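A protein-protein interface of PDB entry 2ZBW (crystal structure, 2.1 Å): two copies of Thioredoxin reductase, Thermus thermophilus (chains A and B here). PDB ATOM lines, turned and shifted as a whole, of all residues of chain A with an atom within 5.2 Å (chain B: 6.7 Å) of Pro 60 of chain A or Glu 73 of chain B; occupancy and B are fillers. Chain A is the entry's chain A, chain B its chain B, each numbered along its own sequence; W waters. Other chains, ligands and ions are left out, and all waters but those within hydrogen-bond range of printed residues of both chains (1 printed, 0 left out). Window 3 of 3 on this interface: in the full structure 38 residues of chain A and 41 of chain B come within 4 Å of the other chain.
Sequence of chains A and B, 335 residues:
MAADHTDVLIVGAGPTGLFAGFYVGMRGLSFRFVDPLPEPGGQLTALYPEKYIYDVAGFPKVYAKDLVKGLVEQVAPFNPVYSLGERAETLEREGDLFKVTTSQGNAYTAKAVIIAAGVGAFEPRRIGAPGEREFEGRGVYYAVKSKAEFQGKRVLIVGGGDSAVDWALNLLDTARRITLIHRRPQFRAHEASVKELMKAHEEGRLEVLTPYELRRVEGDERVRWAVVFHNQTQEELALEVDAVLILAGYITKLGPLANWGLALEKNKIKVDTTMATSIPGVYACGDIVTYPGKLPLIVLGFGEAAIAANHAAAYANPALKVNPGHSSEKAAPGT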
ATOM      1  N   ILE A  53       3.189   0.148 -16.813  1.00  0.00           N
ATOM      2  CA  ILE A  53       4.033   0.659 -15.739  1.00  0.00           C
ATOM      3  C   ILE A  53       3.020   1.038 -14.663  1.00  0.00           C
ATOM      4  O   ILE A  53       1.982   1.617 -14.980  1.00  0.00           O
ATOM      5  CB  ILE A  53       4.812   1.912 -16.181  1.00  0.00           C
ATOM      6  CG1 ILE A  53       5.791   1.554 -17.306  1.00  0.00           C
ATOM      7  CG2 ILE A  53       5.542   2.499 -14.995  1.00  0.00           C
ATOM      8  CD1 ILE A  53       6.442   2.771 -17.971  1.00  0.00           C
ATOM      9  N   TYR A  54       3.314   0.709 -13.408  1.00  0.00           N
ATOM     10  CA  TYR A  54       2.397   0.981 -12.307  1.00  0.00           C
ATOM     11  C   TYR A  54       2.870   2.012 -11.286  1.00  0.00           C
ATOM     12  O   TYR A  54       2.074   2.486 -10.484  1.00  0.00           O
ATOM     13  CB  TYR A  54       2.091  -0.329 -11.558  1.00  0.00           C
ATOM     14  CG  TYR A  54       1.550  -1.433 -12.435  1.00  0.00           C
ATOM     15  CD1 TYR A  54       0.276  -1.343 -12.995  1.00  0.00           C
ATOM     16  CD2 TYR A  54       2.319  -2.563 -12.724  1.00  0.00           C
ATOM     17  CE1 TYR A  54      -0.223  -2.352 -13.826  1.00  0.00           C
ATOM     18  CE2 TYR A  54       1.827  -3.578 -13.555  1.00  0.00           C
ATOM     19  CZ  TYR A  54       0.561  -3.461 -14.102  1.00  0.00           C
ATOM     20  OH  TYR A  54       0.083  -4.434 -14.944  1.00  0.00           O
ATOM     21  N   GLY A  58       0.407   9.288 -10.469  1.00  0.00           N
ATOM     22  CA  GLY A  58      -0.788   9.748 -11.154  1.00  0.00           C
ATOM     23  C   GLY A  58      -1.347   8.770 -12.175  1.00  0.00           C
ATOM     24  O   GLY A  58      -2.428   8.977 -12.715  1.00  0.00           O
ATOM     25  N   PHE A  59      -0.612   7.701 -12.446  1.00  0.00           N
ATOM     26  CA  PHE A  59      -1.058   6.709 -13.414  1.00  0.00           C
ATOM     27  C   PHE A  59      -1.319   5.351 -12.764  1.00  0.00           C
ATOM     28  O   PHE A  59      -0.380   4.616 -12.471  1.00  0.00           O
ATOM     29  CB  PHE A  59       0.000   6.527 -14.500  1.00  0.00           C
ATOM     30  CG  PHE A  59       0.155   7.705 -15.406  1.00  0.00           C
ATOM     31  CD1 PHE A  59      -0.755   7.936 -16.434  1.00  0.00           C
ATOM     32  CD2 PHE A  59       1.226   8.581 -15.246  1.00  0.00           C
ATOM     33  CE1 PHE A  59      -0.598   9.023 -17.293  1.00  0.00           C
ATOM     34  CE2 PHE A  59       1.395   9.671 -16.099  1.00  0.00           C
ATOM     35  CZ  PHE A  59       0.480   9.891 -17.126  1.00  0.00           C
ATOM     36  N   PRO A  60      -2.594   5.005 -12.517  1.00  0.00           N
ATOM     37  CA  PRO A  60      -2.863   3.699 -11.904  1.00  0.00           C
ATOM     38  C   PRO A  60      -2.131   2.637 -12.729  1.00  0.00           C
ATOM     39  O   PRO A  60      -1.702   1.604 -12.219  1.00  0.00           O
ATOM     40  CB  PRO A  60      -4.380   3.593 -11.995  1.00  0.00           C
ATOM     41  CG  PRO A  60      -4.799   5.004 -11.728  1.00  0.00           C
ATOM     42  CD  PRO A  60      -3.828   5.809 -12.600  1.00  0.00           C
ATOM     43  N   LYS A  61      -1.998   2.927 -14.018  1.00  0.00           N
ATOM     44  CA  LYS A  61      -1.281   2.081 -14.955  1.00  0.00           C
ATOM     45  C   LYS A  61      -1.223   2.816 -16.287  1.00  0.00           C
ATOM     46  O   LYS A  61      -2.196   3.457 -16.698  1.00  0.00           O
ATOM     47  CB  LYS A  61      -1.968   0.722 -15.139  1.00  0.00           C
ATOM     48  CG  LYS A  61      -3.275   0.754 -15.899  1.00  0.00           C
ATOM     49  CD  LYS A  61      -3.756  -0.665 -16.154  1.00  0.00           C
ATOM     50  CE  LYS A  61      -5.044  -0.689 -16.943  1.00  0.00           C
ATOM     51  NZ  LYS A  61      -5.442  -2.089 -17.266  1.00  0.00           N
ATOM     52  N   VAL A  62      -0.075   2.720 -16.948  1.00  0.00           N
ATOM     53  CA  VAL A  62       0.140   3.362 -18.236  1.00  0.00           C
ATOM     54  C   VAL A  62       1.181   2.573 -19.027  1.00  0.00           C
ATOM     55  O   VAL A  62       2.247   2.238 -18.512  1.00  0.00           O
ATOM     56  CB  VAL A  62       0.627   4.835 -18.053  1.00  0.00           C
ATOM     57  CG1 VAL A  62       2.002   4.864 -17.388  1.00  0.00           C
ATOM     58  CG2 VAL A  62       0.670   5.542 -19.395  1.00  0.00           C
ATOM     59  N   PHE B  22       1.365   4.966  -1.577  1.00  0.00           N
ATOM     60  CA  PHE B  22       1.281   4.006  -2.661  1.00  0.00           C
ATOM     61  C   PHE B  22       2.501   3.110  -2.657  1.00  0.00           C
ATOM     62  O   PHE B  22       2.369   1.886  -2.730  1.00  0.00           O
ATOM     63  CB  PHE B  22       1.193   4.711  -4.015  1.00  0.00           C
ATOM     64  CG  PHE B  22       1.524   3.819  -5.180  1.00  0.00           C
ATOM     65  CD1 PHE B  22       0.604   2.891  -5.649  1.00  0.00           C
ATOM     66  CD2 PHE B  22       2.770   3.895  -5.794  1.00  0.00           C
ATOM     67  CE1 PHE B  22       0.917   2.050  -6.711  1.00  0.00           C
ATOM     68  CE2 PHE B  22       3.093   3.059  -6.856  1.00  0.00           C
ATOM     69  CZ  PHE B  22       2.161   2.133  -7.314  1.00  0.00           C
ATOM     70  N   VAL B  68      -5.461  14.397  -8.066  1.00  0.00           N
ATOM     71  CA  VAL B  68      -5.734  13.829  -6.758  1.00  0.00           C
ATOM     72  C   VAL B  68      -6.512  12.522  -6.933  1.00  0.00           C
ATOM     73  O   VAL B  68      -6.178  11.506  -6.326  1.00  0.00           O
ATOM     74  CB  VAL B  68      -6.570  14.792  -5.883  1.00  0.00           C
ATOM     75  CG1 VAL B  68      -6.917  14.118  -4.564  1.00  0.00           C
ATOM     76  CG2 VAL B  68      -5.790  16.087  -5.635  1.00  0.00           C
ATOM     77  N   LYS B  69      -7.550  12.551  -7.760  1.00  0.00           N
ATOM     78  CA  LYS B  69      -8.342  11.357  -7.999  1.00  0.00           C
ATOM     79  C   LYS B  69      -7.460  10.232  -8.519  1.00  0.00           C
ATOM     80  O   LYS B  69      -7.613   9.083  -8.121  1.00  0.00           O
ATOM     81  CB  LYS B  69      -9.466  11.646  -8.997  1.00  0.00           C
ATOM     82  CG  LYS B  69     -10.677  12.296  -8.363  1.00  0.00           C
ATOM     83  CD  LYS B  69     -11.794  12.536  -9.376  1.00  0.00           C
ATOM     84  CE  LYS B  69     -13.111  12.860  -8.673  1.00  0.00           C
ATOM     85  NZ  LYS B  69     -12.977  13.979  -7.692  1.00  0.00           N
ATOM     86  N   GLY B  70      -6.537  10.574  -9.408  1.00  0.00           N
ATOM     87  CA  GLY B  70      -5.634   9.580  -9.964  1.00  0.00           C
ATOM     88  C   GLY B  70      -4.765   8.947  -8.893  1.00  0.00           C
ATOM     89  O   GLY B  70      -4.608   7.723  -8.846  1.00  0.00           O
ATOM     90  N   LEU B  71      -4.202   9.781  -8.023  1.00  0.00           N
ATOM     91  CA  LEU B  71      -3.352   9.298  -6.944  1.00  0.00           C
ATOM     92  C   LEU B  71      -4.151   8.448  -5.952  1.00  0.00           C
ATOM     93  O   LEU B  71      -3.669   7.422  -5.474  1.00  0.00           O
ATOM     94  CB  LEU B  71      -2.701  10.482  -6.221  1.00  0.00           C
ATOM     95  CG  LEU B  71      -1.673  11.258  -7.057  1.00  0.00           C
ATOM     96  CD1 LEU B  71      -1.334  12.579  -6.376  1.00  0.00           C
ATOM     97  CD2 LEU B  71      -0.412  10.400  -7.236  1.00  0.00           C
ATOM     98  N   VAL B  72      -5.373   8.877  -5.643  1.00  0.00           N
ATOM     99  CA  VAL B  72      -6.216   8.137  -4.708  1.00  0.00           C
ATOM    100  C   VAL B  72      -6.522   6.742  -5.267  1.00  0.00           C
ATOM    101  O   VAL B  72      -6.439   5.747  -4.553  1.00  0.00           O
ATOM    102  CB  VAL B  72      -7.534   8.904  -4.420  1.00  0.00           C
ATOM    103  CG1 VAL B  72      -8.525   8.004  -3.675  1.00  0.00           C
ATOM    104  CG2 VAL B  72      -7.226  10.129  -3.567  1.00  0.00           C
ATOM    105  N   GLU B  73      -6.846   6.679  -6.554  1.00  0.00           N
ATOM    106  CA  GLU B  73      -7.147   5.412  -7.211  1.00  0.00           C
ATOM    107  C   GLU B  73      -5.904   4.532  -7.281  1.00  0.00           C
ATOM    108  O   GLU B  73      -5.983   3.306  -7.186  1.00  0.00           O
ATOM    109  CB  GLU B  73      -7.660   5.663  -8.624  1.00  0.00           C
ATOM    110  CG  GLU B  73      -8.173   4.417  -9.317  1.00  0.00           C
ATOM    111  CD  GLU B  73      -8.686   4.711 -10.710  1.00  0.00           C
ATOM    112  OE1 GLU B  73      -9.340   5.766 -10.884  1.00  0.00           O
ATOM    113  OE2 GLU B  73      -8.446   3.888 -11.621  1.00  0.00           O
ATOM    114  N   GLN B  74      -4.753   5.172  -7.437  1.00  0.00           N
ATOM    115  CA  GLN B  74      -3.485   4.463  -7.526  1.00  0.00           C
ATOM    116  C   GLN B  74      -3.090   3.820  -6.197  1.00  0.00           C
ATOM    117  O   GLN B  74      -2.458   2.769  -6.176  1.00  0.00           O
ATOM    118  CB  GLN B  74      -2.395   5.431  -7.999  1.00  0.00           C
ATOM    119  CG  GLN B  74      -0.997   4.860  -8.048  1.00  0.00           C
ATOM    120  CD  GLN B  74      -0.045   5.762  -8.822  1.00  0.00           C
ATOM    121  OE1 GLN B  74       0.008   6.974  -8.591  1.00  0.00           O
ATOM    122  NE2 GLN B  74       0.709   5.174  -9.746  1.00  0.00           N
ATOM    123  N   VAL B  75      -3.459   4.446  -5.089  1.00  0.00           N
ATOM    124  CA  VAL B  75      -3.122   3.889  -3.782  1.00  0.00           C
ATOM    125  C   VAL B  75      -4.162   2.862  -3.312  1.00  0.00           C
ATOM    126  O   VAL B  75      -3.839   1.932  -2.567  1.00  0.00           O
ATOM    127  CB  VAL B  75      -3.023   4.994  -2.713  1.00  0.00           C
ATOM    128  CG1 VAL B  75      -2.014   6.047  -3.130  1.00  0.00           C
ATOM    129  CG2 VAL B  75      -4.369   5.633  -2.508  1.00  0.00           C
ATOM    130  N   ALA B  76      -5.398   3.039  -3.771  1.00  0.00           N
ATOM    131  CA  ALA B  76      -6.534   2.197  -3.395  1.00  0.00           C
ATOM    132  C   ALA B  76      -6.337   0.681  -3.314  1.00  0.00           C
ATOM    133  O   ALA B  76      -6.757   0.057  -2.341  1.00  0.00           O
ATOM    134  CB  ALA B  76      -7.706   2.504  -4.299  1.00  0.00           C
ATOM    135  N   PRO B  77      -5.689   0.066  -4.321  1.00  0.00           N
ATOM    136  CA  PRO B  77      -5.499  -1.388  -4.265  1.00  0.00           C
ATOM    137  C   PRO B  77      -4.801  -1.878  -3.000  1.00  0.00           C
ATOM    138  O   PRO B  77      -4.919  -3.049  -2.635  1.00  0.00           O
ATOM    139  CB  PRO B  77      -4.672  -1.683  -5.516  1.00  0.00           C
ATOM    140  CG  PRO B  77      -4.974  -0.544  -6.430  1.00  0.00           C
ATOM    141  CD  PRO B  77      -5.015   0.634  -5.500  1.00  0.00           C
ATOM    142  N   TYR B  82      -7.416   5.794   5.972  1.00  0.00           N
ATOM    143  CA  TYR B  82      -7.509   7.245   5.959  1.00  0.00           C
ATOM    144  C   TYR B  82      -8.034   7.777   7.291  1.00  0.00           C
ATOM    145  O   TYR B  82      -9.187   7.545   7.649  1.00  0.00           O
ATOM    146  CB  TYR B  82      -8.427   7.695   4.826  1.00  0.00           C
ATOM    147  CG  TYR B  82      -7.795   7.644   3.455  1.00  0.00           C
ATOM    148  CD1 TYR B  82      -6.941   8.661   3.021  1.00  0.00           C
ATOM    149  CD2 TYR B  82      -8.068   6.597   2.579  1.00  0.00           C
ATOM    150  CE1 TYR B  82      -6.385   8.633   1.744  1.00  0.00           C
ATOM    151  CE2 TYR B  82      -7.514   6.563   1.303  1.00  0.00           C
ATOM    152  CZ  TYR B  82      -6.678   7.582   0.891  1.00  0.00           C
ATOM    153  OH  TYR B  82      -6.158   7.561  -0.387  1.00  0.00           O
ATOM    154  N   PRO B 333      -0.642  -3.955  -9.131  1.00  0.00           N
ATOM    155  CA  PRO B 333      -0.854  -3.563  -7.735  1.00  0.00           C
ATOM    156  C   PRO B 333      -2.098  -4.188  -7.091  1.00  0.00           C
ATOM    157  O   PRO B 333      -3.214  -4.069  -7.600  1.00  0.00           O
ATOM    158  CB  PRO B 333      -0.905  -2.029  -7.802  1.00  0.00           C
ATOM    159  CG  PRO B 333      -1.201  -1.734  -9.243  1.00  0.00           C
ATOM    160  CD  PRO B 333      -0.420  -2.773  -9.974  1.00  0.00           C
HETATM  161  O   HOH W   1      -0.497   1.893  -9.886  1.00  0.00           O
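The backbone carbonyl oxygen (O) of Tyr 54 of chain A sits at hydrogen-bond distance from the side-chain amide nitrogen (NE2) of Gln 74 of chain B (3.1 Å).
The backbone carbonyl oxygen of Phe 59 of chain A is in hydrogen-bond range of the side-chain amide nitrogen of Gln 74 of chain B (3.0 Å).
N of Gly 58 of chain A lies within hydrogen-bond range of OE1 of Gln 74 of chain B, at 3.0 Å.
Among the printed residues, merely in contact across the chains: Tyr 54 of chain A with Phe 22 of chain B, Tyr 54 of chain A with Pro 333 of chain B, Gly 58 of chain A with Leu 71 of chain B, Pro 60 of chain A with Gly 70 of chain B and Pro 60 of chain A with Glu 73 of chain B.
Of the printed residues of chain B, Pro 60 of chain A touches Gly 70 and Glu 73.
Val 62 of chain A touches none of the printed residues of chain B.
Of the printed residues of chain A, Phe 22 of chain B touches Tyr 54 (3.2 Å).
Printed residues of chain A within 4 Å of Gly 70 of chain B: Pro 60.
Glu 73 of chain B touches one residue of chain A.
The nearest residue of chain B that does not touch Pro 60 of chain A is Gln 74 of chain B (4.3 Å).
The nearest printed residue of chain A that does not touch Glu 73 of chain B is Lys 61 of chain A (6.9 Å).
The nearest printed residue of chain B that does not touch Phe 59 of chain A is Gly 70 of chain B (5.4 Å).
Of the 13 printed residues of chain B, 6 touch a printed residue of chain A.
Along chain B the printed residues that touch a printed residue of chain A span positions 22 to 333.
Of the 7 printed residues of chain A, 4 touch a printed residue of chain B.
Printed residues of chain A that touch a printed residue of chain B: Tyr 54, Gly 58, Phe 59 and Pro 60.
Hydrophobic or aromatic side chains of chain A within 4 Å of the printed part of chain B: Tyr 54 and Pro 60.
Along chain A the printed residues that touch a printed residue of chain B span positions 54 to 60.
Among the printed residues, 8 pairs touch across the chains.
Among the printed residues, no Asp or Glu carboxylate lies within 4 Å of a Lys or Arg side-chain nitrogen of the other chain.
No position is printed for both chains.
Water W1 lies within hydrogen-bond range of the backbone carbonyl oxygen (O) of Pro 60 of chain A (2.6 Å), the backbone carbonyl oxygen (O) of Tyr 54 of chain A (2.7 Å) and the side-chain amide nitrogen (NE2) of Gln 74 of chain B (3.5 Å).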
